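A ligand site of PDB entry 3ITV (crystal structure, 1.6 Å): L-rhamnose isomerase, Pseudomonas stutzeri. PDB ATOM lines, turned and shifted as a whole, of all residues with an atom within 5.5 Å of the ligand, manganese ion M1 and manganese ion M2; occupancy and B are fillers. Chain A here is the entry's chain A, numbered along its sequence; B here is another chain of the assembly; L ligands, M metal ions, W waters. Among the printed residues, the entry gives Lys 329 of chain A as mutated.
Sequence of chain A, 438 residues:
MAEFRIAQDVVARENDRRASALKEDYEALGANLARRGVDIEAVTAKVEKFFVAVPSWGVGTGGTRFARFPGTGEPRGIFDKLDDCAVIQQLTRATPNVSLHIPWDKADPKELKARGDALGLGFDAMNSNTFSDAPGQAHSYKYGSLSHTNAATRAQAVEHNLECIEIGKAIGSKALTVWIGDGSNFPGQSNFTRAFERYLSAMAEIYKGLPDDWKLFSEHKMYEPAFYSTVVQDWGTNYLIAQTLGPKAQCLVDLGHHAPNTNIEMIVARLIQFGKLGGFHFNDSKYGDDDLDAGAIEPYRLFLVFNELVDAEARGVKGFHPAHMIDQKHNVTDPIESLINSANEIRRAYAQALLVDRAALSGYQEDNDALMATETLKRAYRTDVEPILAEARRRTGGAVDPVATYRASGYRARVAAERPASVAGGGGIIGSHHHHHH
An oxygen (O5) of the ligand lies within hydrogen-bond range of the side-chain amino group of Lys 329 (2.6 Å). The side-chain amino group of Lys 221 sits close to an oxygen (O1) of the ligand (2.7 Å). An oxygen (O4) of the ligand is in hydrogen-bond range of a ring nitrogen (NE2) of His 101 (3.1 Å).
NZ of Lys 329 is in salt-bridge range of OD1 of Asp 327 (2.7 Å). The side-chain carboxylate (OD1) of Asp 327 lies within hydrogen-bond range of the indole nitrogen (NE1) of Trp 57, at 3.0 Å. ND2 of Asn 283 sits at hydrogen-bond distance from O of Asp 327. The side-chain carboxylate of Asp 289 sits close to the side-chain amino group of Lys 221 (3.1 Å). The guanidinium group (NH2) of Arg 65 of chain B lies within hydrogen-bond range of the backbone carbonyl oxygen (O) of Asp 289 (3.1 Å). OD1 of Asp 254 is in hydrogen-bond range of ND2 of Asn 283 (2.8 Å). NZ of Lys 329 is in salt-bridge range of OD2 of Asp 291 (3.1 Å). NZ of Lys 221 is in salt-bridge range of OE1 of Glu 224 (3.1 Å).
NE1 of Trp 57 touches C6 of the ligand (3.7 Å). Trp 104 touches the ligand (CH2 to O6, 3.96 Å). Trp 179 touches the ligand. Phe 66 of chain B touches the ligand (CZ to O1, 3.4 Å). Hydrophobic or aromatic side chains within 4 Å of the ligand: Trp 57, His 101, Trp 104, Trp 179, His 257, His 281 and Phe 66 of chain B. Of the 21 residues printed, 13 come within 4 Å of the ligand.
Five residues have an atom within 4 Å of manganese ion M1: Glu 219, Asp 254, His 257, His 281 and Asp 327. The nearest printed residue that does not touch manganese ion M1 is Leu 252 (5.0 Å).
Residues that only touch manganese ion M2: Lys 221 and Asp 291. Five residues have an atom within 4 Å of manganese ion M2: Lys 221, Asp 254, His 257, Asp 289 and Asp 291.
Manganese ion M1 is bound by OD2 of Asp 327 (2.0 Å), OE2 of Glu 219 (2.1 Å), OD2 of Asp 254 (2.2 Å), O2 of the ligand (2.2 Å), ND1 of His 281 (2.3 Å) and O3 of the ligand (2.3 Å).
Manganese ion M2 is bound by water W2, 1.8 Å away. Manganese ion M2 is bound by O1 of the ligand, at 2.0 Å. Manganese ion M2 is bound by a ring nitrogen (NE2) of His 257 (2.0 Å). Manganese ion M2 is bound by water W1, 2.1 Å away. The side-chain carboxylate (OD2) of Asp 289 is bound to manganese ion M2. An oxygen (O2) of the ligand is bound to manganese ion M2 (2.3 Å).
Water W1 lies within hydrogen-bond range of the side-chain amino group (NZ) of Lys 329 (2.5 Å), the side-chain carboxylate (OD2) of Asp 291 (2.8 Å) and an oxygen (O5) of the ligand (3.0 Å). Water W2 lies within hydrogen-bond range of OD1 of Asp 289 (2.4 Å) and OD2 of Asp 291 (3.4 Å). Water W3 lies within hydrogen-bond range of O4 of the ligand (2.6 Å) and OD1 of Asn 127 (2.7 Å).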
ATOM      1  N   TRP A  57      10.122  -1.936  -0.179  1.00  0.00           N
ATOM      2  CA  TRP A  57       8.738  -2.216   0.159  1.00  0.00           C
ATOM      3  C   TRP A  57       7.726  -1.365  -0.614  1.00  0.00           C
ATOM      4  O   TRP A  57       6.518  -1.570  -0.496  1.00  0.00           O
ATOM      5  CB  TRP A  57       8.527  -2.038   1.665  1.00  0.00           C
ATOM      6  CG  TRP A  57       8.765  -0.655   2.170  1.00  0.00           C
ATOM      7  CD1 TRP A  57       7.858   0.358   2.269  1.00  0.00           C
ATOM      8  CD2 TRP A  57      10.007  -0.122   2.650  1.00  0.00           C
ATOM      9  NE1 TRP A  57       8.451   1.484   2.791  1.00  0.00           N
ATOM     10  CE2 TRP A  57       9.773   1.223   3.029  1.00  0.00           C
ATOM     11  CE3 TRP A  57      11.297  -0.645   2.800  1.00  0.00           C
ATOM     12  CZ2 TRP A  57      10.769   2.041   3.551  1.00  0.00           C
ATOM     13  CZ3 TRP A  57      12.298   0.169   3.314  1.00  0.00           C
ATOM     14  CH2 TRP A  57      12.033   1.501   3.681  1.00  0.00           C
ATOM     15  N   HIS A 101      14.453  -3.759   3.985  1.00  0.00           N
ATOM     16  CA  HIS A 101      13.685  -3.940   5.211  1.00  0.00           C
ATOM     17  C   HIS A 101      13.803  -5.415   5.599  1.00  0.00           C
ATOM     18  O   HIS A 101      13.509  -6.292   4.801  1.00  0.00           O
ATOM     19  CB  HIS A 101      12.228  -3.551   4.987  1.00  0.00           C
ATOM     20  CG  HIS A 101      11.585  -2.868   6.158  1.00  0.00           C
ATOM     21  ND1 HIS A 101      11.422  -3.496   7.374  1.00  0.00           N
ATOM     22  CD2 HIS A 101      11.105  -1.616   6.300  1.00  0.00           C
ATOM     23  CE1 HIS A 101      10.857  -2.646   8.219  1.00  0.00           C
ATOM     24  NE2 HIS A 101      10.653  -1.499   7.596  1.00  0.00           N
ATOM     25  N   TRP A 104      11.636  -8.810   5.660  1.00  0.00           N
ATOM     26  CA  TRP A 104      10.999  -8.903   4.356  1.00  0.00           C
ATOM     27  C   TRP A 104      12.006  -9.224   3.256  1.00  0.00           C
ATOM     28  O   TRP A 104      11.768 -10.079   2.409  1.00  0.00           O
ATOM     29  CB  TRP A 104      10.270  -7.604   3.973  1.00  0.00           C
ATOM     30  CG  TRP A 104       9.124  -7.231   4.863  1.00  0.00           C
ATOM     31  CD1 TRP A 104       8.375  -8.075   5.638  1.00  0.00           C
ATOM     32  CD2 TRP A 104       8.569  -5.924   5.041  1.00  0.00           C
ATOM     33  NE1 TRP A 104       7.390  -7.363   6.290  1.00  0.00           N
ATOM     34  CE2 TRP A 104       7.498  -6.036   5.943  1.00  0.00           C
ATOM     35  CE3 TRP A 104       8.894  -4.654   4.519  1.00  0.00           C
ATOM     36  CZ2 TRP A 104       6.724  -4.934   6.340  1.00  0.00           C
ATOM     37  CZ3 TRP A 104       8.126  -3.558   4.922  1.00  0.00           C
ATOM     38  CH2 TRP A 104       7.062  -3.713   5.830  1.00  0.00           C
ATOM     39  N   ASN A 127      16.572  -1.222   7.506  1.00  0.00           N
ATOM     40  CA  ASN A 127      15.372  -0.968   8.292  1.00  0.00           C
ATOM     41  C   ASN A 127      15.009  -2.242   9.043  1.00  0.00           C
ATOM     42  O   ASN A 127      14.872  -3.309   8.443  1.00  0.00           O
ATOM     43  CB  ASN A 127      14.209  -0.575   7.368  1.00  0.00           C
ATOM     44  CG  ASN A 127      14.425   0.746   6.676  1.00  0.00           C
ATOM     45  OD1 ASN A 127      14.026   1.796   7.193  1.00  0.00           O
ATOM     46  ND2 ASN A 127      15.077   0.722   5.522  1.00  0.00           N
ATOM     47  N   SER A 128      14.865  -2.133  10.361  1.00  0.00           N
ATOM     48  CA  SER A 128      14.500  -3.271  11.193  1.00  0.00           C
ATOM     49  C   SER A 128      12.985  -3.379  11.282  1.00  0.00           C
ATOM     50  O   SER A 128      12.271  -2.410  11.025  1.00  0.00           O
ATOM     51  CB  SER A 128      15.107  -3.122  12.592  1.00  0.00           C
ATOM     52  OG  SER A 128      14.720  -1.895  13.193  1.00  0.00           O
ATOM     53  N   PHE A 131       7.615  -4.621  14.465  1.00  0.00           N
ATOM     54  CA  PHE A 131       6.250  -4.138  14.538  1.00  0.00           C
ATOM     55  C   PHE A 131       5.309  -5.211  13.994  1.00  0.00           C
ATOM     56  O   PHE A 131       4.121  -4.978  13.789  1.00  0.00           O
ATOM     57  CB  PHE A 131       6.085  -2.814  13.778  1.00  0.00           C
ATOM     58  CG  PHE A 131       6.614  -2.834  12.369  1.00  0.00           C
ATOM     59  CD1 PHE A 131       5.878  -3.403  11.337  1.00  0.00           C
ATOM     60  CD2 PHE A 131       7.846  -2.251  12.069  1.00  0.00           C
ATOM     61  CE1 PHE A 131       6.358  -3.391  10.021  1.00  0.00           C
ATOM     62  CE2 PHE A 131       8.334  -2.233  10.767  1.00  0.00           C
ATOM     63  CZ  PHE A 131       7.587  -2.807   9.743  1.00  0.00           C
ATOM     64  N   TRP A 179      12.143   2.137  13.318  1.00  0.00           N
ATOM     65  CA  TRP A 179      10.784   2.624  13.500  1.00  0.00           C
ATOM     66  C   TRP A 179      10.023   1.456  14.102  1.00  0.00           C
ATOM     67  O   TRP A 179      10.060   0.343  13.560  1.00  0.00           O
ATOM     68  CB  TRP A 179      10.097   3.021  12.196  1.00  0.00           C
ATOM     69  CG  TRP A 179       8.635   3.319  12.451  1.00  0.00           C
ATOM     70  CD1 TRP A 179       8.125   4.425  13.067  1.00  0.00           C
ATOM     71  CD2 TRP A 179       7.527   2.449  12.221  1.00  0.00           C
ATOM     72  NE1 TRP A 179       6.771   4.292  13.250  1.00  0.00           N
ATOM     73  CE2 TRP A 179       6.376   3.092  12.728  1.00  0.00           C
ATOM     74  CE3 TRP A 179       7.382   1.187  11.626  1.00  0.00           C
ATOM     75  CZ2 TRP A 179       5.098   2.508  12.673  1.00  0.00           C
ATOM     76  CZ3 TRP A 179       6.121   0.603  11.569  1.00  0.00           C
ATOM     77  CH2 TRP A 179       4.990   1.267  12.091  1.00  0.00           C
ATOM     78  N   GLU A 219      12.966   6.924  14.105  1.00  0.00           N
ATOM     79  CA  GLU A 219      11.882   7.601  13.381  1.00  0.00           C
ATOM     80  C   GLU A 219      10.621   7.786  14.231  1.00  0.00           C
ATOM     81  O   GLU A 219       9.998   6.811  14.645  1.00  0.00           O
ATOM     82  CB  GLU A 219      11.560   6.789  12.119  1.00  0.00           C
ATOM     83  CG  GLU A 219      10.388   7.298  11.303  1.00  0.00           C
ATOM     84  CD  GLU A 219      10.170   6.495  10.033  1.00  0.00           C
ATOM     85  OE1 GLU A 219      10.770   5.401   9.897  1.00  0.00           O
ATOM     86  OE2 GLU A 219       9.387   6.935   9.172  1.00  0.00           O
ATOM     87  N   LYS A 221       6.666   9.001  15.131  1.00  0.00           N
ATOM     88  CA  LYS A 221       5.363   8.899  14.476  1.00  0.00           C
ATOM     89  C   LYS A 221       4.294   9.169  15.526  1.00  0.00           C
ATOM     90  O   LYS A 221       4.292   8.539  16.578  1.00  0.00           O
ATOM     91  CB  LYS A 221       5.172   7.509  13.868  1.00  0.00           C
ATOM     92  CG  LYS A 221       3.976   7.412  12.936  1.00  0.00           C
ATOM     93  CD  LYS A 221       3.882   6.051  12.274  1.00  0.00           C
ATOM     94  CE  LYS A 221       2.725   6.014  11.294  1.00  0.00           C
ATOM     95  NZ  LYS A 221       2.570   4.647  10.685  1.00  0.00           N
ATOM     96  N   GLU A 224      -0.484   5.272  14.927  1.00  0.00           N
ATOM     97  CA  GLU A 224      -0.601   4.153  13.989  1.00  0.00           C
ATOM     98  C   GLU A 224       0.716   3.379  13.934  1.00  0.00           C
ATOM     99  O   GLU A 224       1.721   3.879  13.439  1.00  0.00           O
ATOM    100  CB  GLU A 224      -0.966   4.612  12.570  1.00  0.00           C
ATOM    101  CG  GLU A 224      -1.215   3.404  11.653  1.00  0.00           C
ATOM    102  CD  GLU A 224      -1.167   3.727  10.167  1.00  0.00           C
ATOM    103  OE1 GLU A 224      -0.361   4.588   9.770  1.00  0.00           O
ATOM    104  OE2 GLU A 224      -1.931   3.106   9.399  1.00  0.00           O
ATOM    105  N   LEU A 252      15.170  10.764  12.223  1.00  0.00           N
ATOM    106  CA  LEU A 252      14.679  10.675  10.852  1.00  0.00           C
ATOM    107  C   LEU A 252      13.277  11.265  10.833  1.00  0.00           C
ATOM    108  O   LEU A 252      12.435  10.931  11.661  1.00  0.00           O
ATOM    109  CB  LEU A 252      14.666   9.220  10.372  1.00  0.00           C
ATOM    110  CG  LEU A 252      14.310   9.032   8.905  1.00  0.00           C
ATOM    111  CD1 LEU A 252      15.176   7.946   8.278  1.00  0.00           C
ATOM    112  CD2 LEU A 252      12.844   8.708   8.777  1.00  0.00           C
ATOM    113  N   ASP A 254       9.841  11.683   8.822  1.00  0.00           N
ATOM    114  CA  ASP A 254       8.953  11.154   7.791  1.00  0.00           C
ATOM    115  C   ASP A 254       7.843  12.191   7.717  1.00  0.00           C
ATOM    116  O   ASP A 254       7.130  12.418   8.696  1.00  0.00           O
ATOM    117  CB  ASP A 254       8.405   9.782   8.209  1.00  0.00           C
ATOM    118  CG  ASP A 254       7.554   9.152   7.128  1.00  0.00           C
ATOM    119  OD1 ASP A 254       6.630   9.824   6.631  1.00  0.00           O
ATOM    120  OD2 ASP A 254       7.783   7.973   6.770  1.00  0.00           O
ATOM    121  N   HIS A 257       4.187  11.843   9.332  1.00  0.00           N
ATOM    122  CA  HIS A 257       4.092  11.408  10.728  1.00  0.00           C
ATOM    123  C   HIS A 257       3.833  12.496  11.765  1.00  0.00           C
ATOM    124  O   HIS A 257       4.145  12.326  12.935  1.00  0.00           O
ATOM    125  CB  HIS A 257       5.370  10.671  11.113  1.00  0.00           C
ATOM    126  CG  HIS A 257       5.558   9.361  10.414  1.00  0.00           C
ATOM    127  ND1 HIS A 257       6.512   8.444  10.801  1.00  0.00           N
ATOM    128  CD2 HIS A 257       4.896   8.799   9.371  1.00  0.00           C
ATOM    129  CE1 HIS A 257       6.435   7.376  10.031  1.00  0.00           C
ATOM    130  NE2 HIS A 257       5.458   7.575   9.155  1.00  0.00           N
ATOM    131  N   HIS A 281      12.176  10.728   5.128  1.00  0.00           N
ATOM    132  CA  HIS A 281      11.364   9.698   4.505  1.00  0.00           C
ATOM    133  C   HIS A 281      10.346  10.576   3.803  1.00  0.00           C
ATOM    134  O   HIS A 281       9.442  11.139   4.432  1.00  0.00           O
ATOM    135  CB  HIS A 281      10.686   8.804   5.536  1.00  0.00           C
ATOM    136  CG  HIS A 281      11.445   7.548   5.849  1.00  0.00           C
ATOM    137  ND1 HIS A 281      10.887   6.488   6.529  1.00  0.00           N
ATOM    138  CD2 HIS A 281      12.726   7.187   5.569  1.00  0.00           C
ATOM    139  CE1 HIS A 281      11.791   5.530   6.656  1.00  0.00           C
ATOM    140  NE2 HIS A 281      12.909   5.921   6.082  1.00  0.00           N
ATOM    141  N   ASN A 283       7.318  11.636   1.206  1.00  0.00           N
ATOM    142  CA  ASN A 283       6.003  11.171   0.770  1.00  0.00           C
ATOM    143  C   ASN A 283       5.081  12.368   0.939  1.00  0.00           C
ATOM    144  O   ASN A 283       5.521  13.437   1.389  1.00  0.00           O
ATOM    145  CB  ASN A 283       5.522  10.007   1.646  1.00  0.00           C
ATOM    146  CG  ASN A 283       5.650  10.278   3.142  1.00  0.00           C
ATOM    147  OD1 ASN A 283       5.113  11.271   3.643  1.00  0.00           O
ATOM    148  ND2 ASN A 283       6.360   9.408   3.858  1.00  0.00           N
ATOM    149  N   ASP A 289      -0.953   9.397   7.931  1.00  0.00           N
ATOM    150  CA  ASP A 289       0.273   8.903   7.327  1.00  0.00           C
ATOM    151  C   ASP A 289      -0.157   8.198   6.042  1.00  0.00           C
ATOM    152  O   ASP A 289      -0.050   6.978   5.907  1.00  0.00           O
ATOM    153  CB  ASP A 289       0.982   7.936   8.267  1.00  0.00           C
ATOM    154  CG  ASP A 289       2.313   7.472   7.731  1.00  0.00           C
ATOM    155  OD1 ASP A 289       2.956   8.256   6.992  1.00  0.00           O
ATOM    156  OD2 ASP A 289       2.732   6.336   8.060  1.00  0.00           O
ATOM    157  N   ASP A 291       1.090   8.170   3.058  1.00  0.00           N
ATOM    158  CA  ASP A 291       2.167   7.608   2.235  1.00  0.00           C
ATOM    159  C   ASP A 291       1.976   7.762   0.731  1.00  0.00           C
ATOM    160  O   ASP A 291       2.323   6.862  -0.043  1.00  0.00           O
ATOM    161  CB  ASP A 291       2.373   6.131   2.586  1.00  0.00           C
ATOM    162  CG  ASP A 291       3.025   5.933   3.943  1.00  0.00           C
ATOM    163  OD1 ASP A 291       3.936   6.724   4.265  1.00  0.00           O
ATOM    164  OD2 ASP A 291       2.632   5.009   4.684  1.00  0.00           O
ATOM    165  N   ASP A 327       9.603   7.014   1.294  1.00  0.00           N
ATOM    166  CA  ASP A 327       8.883   5.999   2.051  1.00  0.00           C
ATOM    167  C   ASP A 327       7.435   6.187   1.655  1.00  0.00           C
ATOM    168  O   ASP A 327       6.724   7.007   2.222  1.00  0.00           O
ATOM    169  CB  ASP A 327       9.024   6.172   3.565  1.00  0.00           C
ATOM    170  CG  ASP A 327       8.282   5.085   4.336  1.00  0.00           C
ATOM    171  OD1 ASP A 327       7.645   4.224   3.698  1.00  0.00           O
ATOM    172  OD2 ASP A 327       8.336   5.096   5.591  1.00  0.00           O
ATOM    173  N   LYS A 329       3.736   4.120  -0.207  1.00  0.00           N
ATOM    174  CA  LYS A 329       2.995   2.909  -0.479  1.00  0.00           C
ATOM    175  C   LYS A 329       2.117   3.284  -1.662  1.00  0.00           C
ATOM    176  O   LYS A 329       1.492   4.351  -1.672  1.00  0.00           O
ATOM    177  CB  LYS A 329       2.136   2.486   0.715  1.00  0.00           C
ATOM    178  CG  LYS A 329       2.922   1.868   1.866  1.00  0.00           C
ATOM    179  CD  LYS A 329       3.784   2.894   2.575  1.00  0.00           C
ATOM    180  CE  LYS A 329       4.491   2.284   3.777  1.00  0.00           C
ATOM    181  NZ  LYS A 329       5.196   3.326   4.564  1.00  0.00           N
ATOM    182  N   ARG B  65      -2.642  -2.036   9.082  1.00  0.00           N
ATOM    183  CA  ARG B  65      -1.981  -2.403   7.842  1.00  0.00           C
ATOM    184  C   ARG B  65      -0.583  -2.949   8.116  1.00  0.00           C
ATOM    185  O   ARG B  65       0.045  -3.544   7.236  1.00  0.00           O
ATOM    186  CB  ARG B  65      -1.888  -1.217   6.887  1.00  0.00           C
ATOM    187  CG  ARG B  65      -1.216   0.009   7.485  1.00  0.00           C
ATOM    188  CD  ARG B  65      -1.013   1.090   6.423  1.00  0.00           C
ATOM    189  NE  ARG B  65      -0.484   2.312   7.007  1.00  0.00           N
ATOM    190  CZ  ARG B  65       0.355   3.130   6.394  1.00  0.00           C
ATOM    191  NH1 ARG B  65       0.786   2.863   5.165  1.00  0.00           N
ATOM    192  NH2 ARG B  65       0.794   4.218   7.014  1.00  0.00           N
ATOM    193  N   PHE B  66      -0.097  -2.764   9.344  1.00  0.00           N
ATOM    194  CA  PHE B  66       1.232  -3.237   9.720  1.00  0.00           C
ATOM    195  C   PHE B  66       1.241  -4.671  10.227  1.00  0.00           C
ATOM    196  O   PHE B  66       2.190  -5.421   9.960  1.00  0.00           O
ATOM    197  CB  PHE B  66       1.838  -2.318  10.772  1.00  0.00           C
ATOM    198  CG  PHE B  66       2.150  -0.951  10.268  1.00  0.00           C
ATOM    199  CD1 PHE B  66       3.208  -0.755   9.389  1.00  0.00           C
ATOM    200  CD2 PHE B  66       1.363   0.136  10.629  1.00  0.00           C
ATOM    201  CE1 PHE B  66       3.473   0.510   8.862  1.00  0.00           C
ATOM    202  CE2 PHE B  66       1.618   1.396  10.110  1.00  0.00           C
ATOM    203  CZ  PHE B  66       2.675   1.581   9.222  1.00  0.00           C
HETATM  204  C1  LIG L   1       5.818   3.446   9.365  1.00  0.00           C
HETATM  205  O1  LIG L   1       4.696   4.273   9.099  1.00  0.00           O
HETATM  206  C2  LIG L   1       7.053   4.052   8.727  1.00  0.00           C
HETATM  207  O2  LIG L   1       6.993   5.138   8.165  1.00  0.00           O
HETATM  208  C3  LIG L   1       8.387   3.310   8.812  1.00  0.00           C
HETATM  209  O3  LIG L   1       9.383   4.026   8.093  1.00  0.00           O
HETATM  210  C4  LIG L   1       8.242   1.896   8.237  1.00  0.00           C
HETATM  211  O4  LIG L   1       9.409   1.134   8.549  1.00  0.00           O
HETATM  212  C5  LIG L   1       8.024   1.919   6.731  1.00  0.00           C
HETATM  213  O5  LIG L   1       6.958   2.794   6.406  1.00  0.00           O
HETATM  214  C6  LIG L   1       7.700   0.513   6.237  1.00  0.00           C
HETATM  215  O6  LIG L   1       6.466   0.086   6.787  1.00  0.00           O
HETATM  216 MN    MN M   1       8.813   6.087   7.307  1.00  0.00          MN
HETATM  217 MN    MN M   2       4.846   5.973   8.037  1.00  0.00          MN
HETATM  218  O   HOH W   1       4.434   4.377   6.678  1.00  0.00           O
HETATM  219  O   HOH W   2       4.855   6.806   6.466  1.00  0.00           O
HETATM  220  O   HOH W   3      11.909   1.919   8.933  1.00  0.00           O
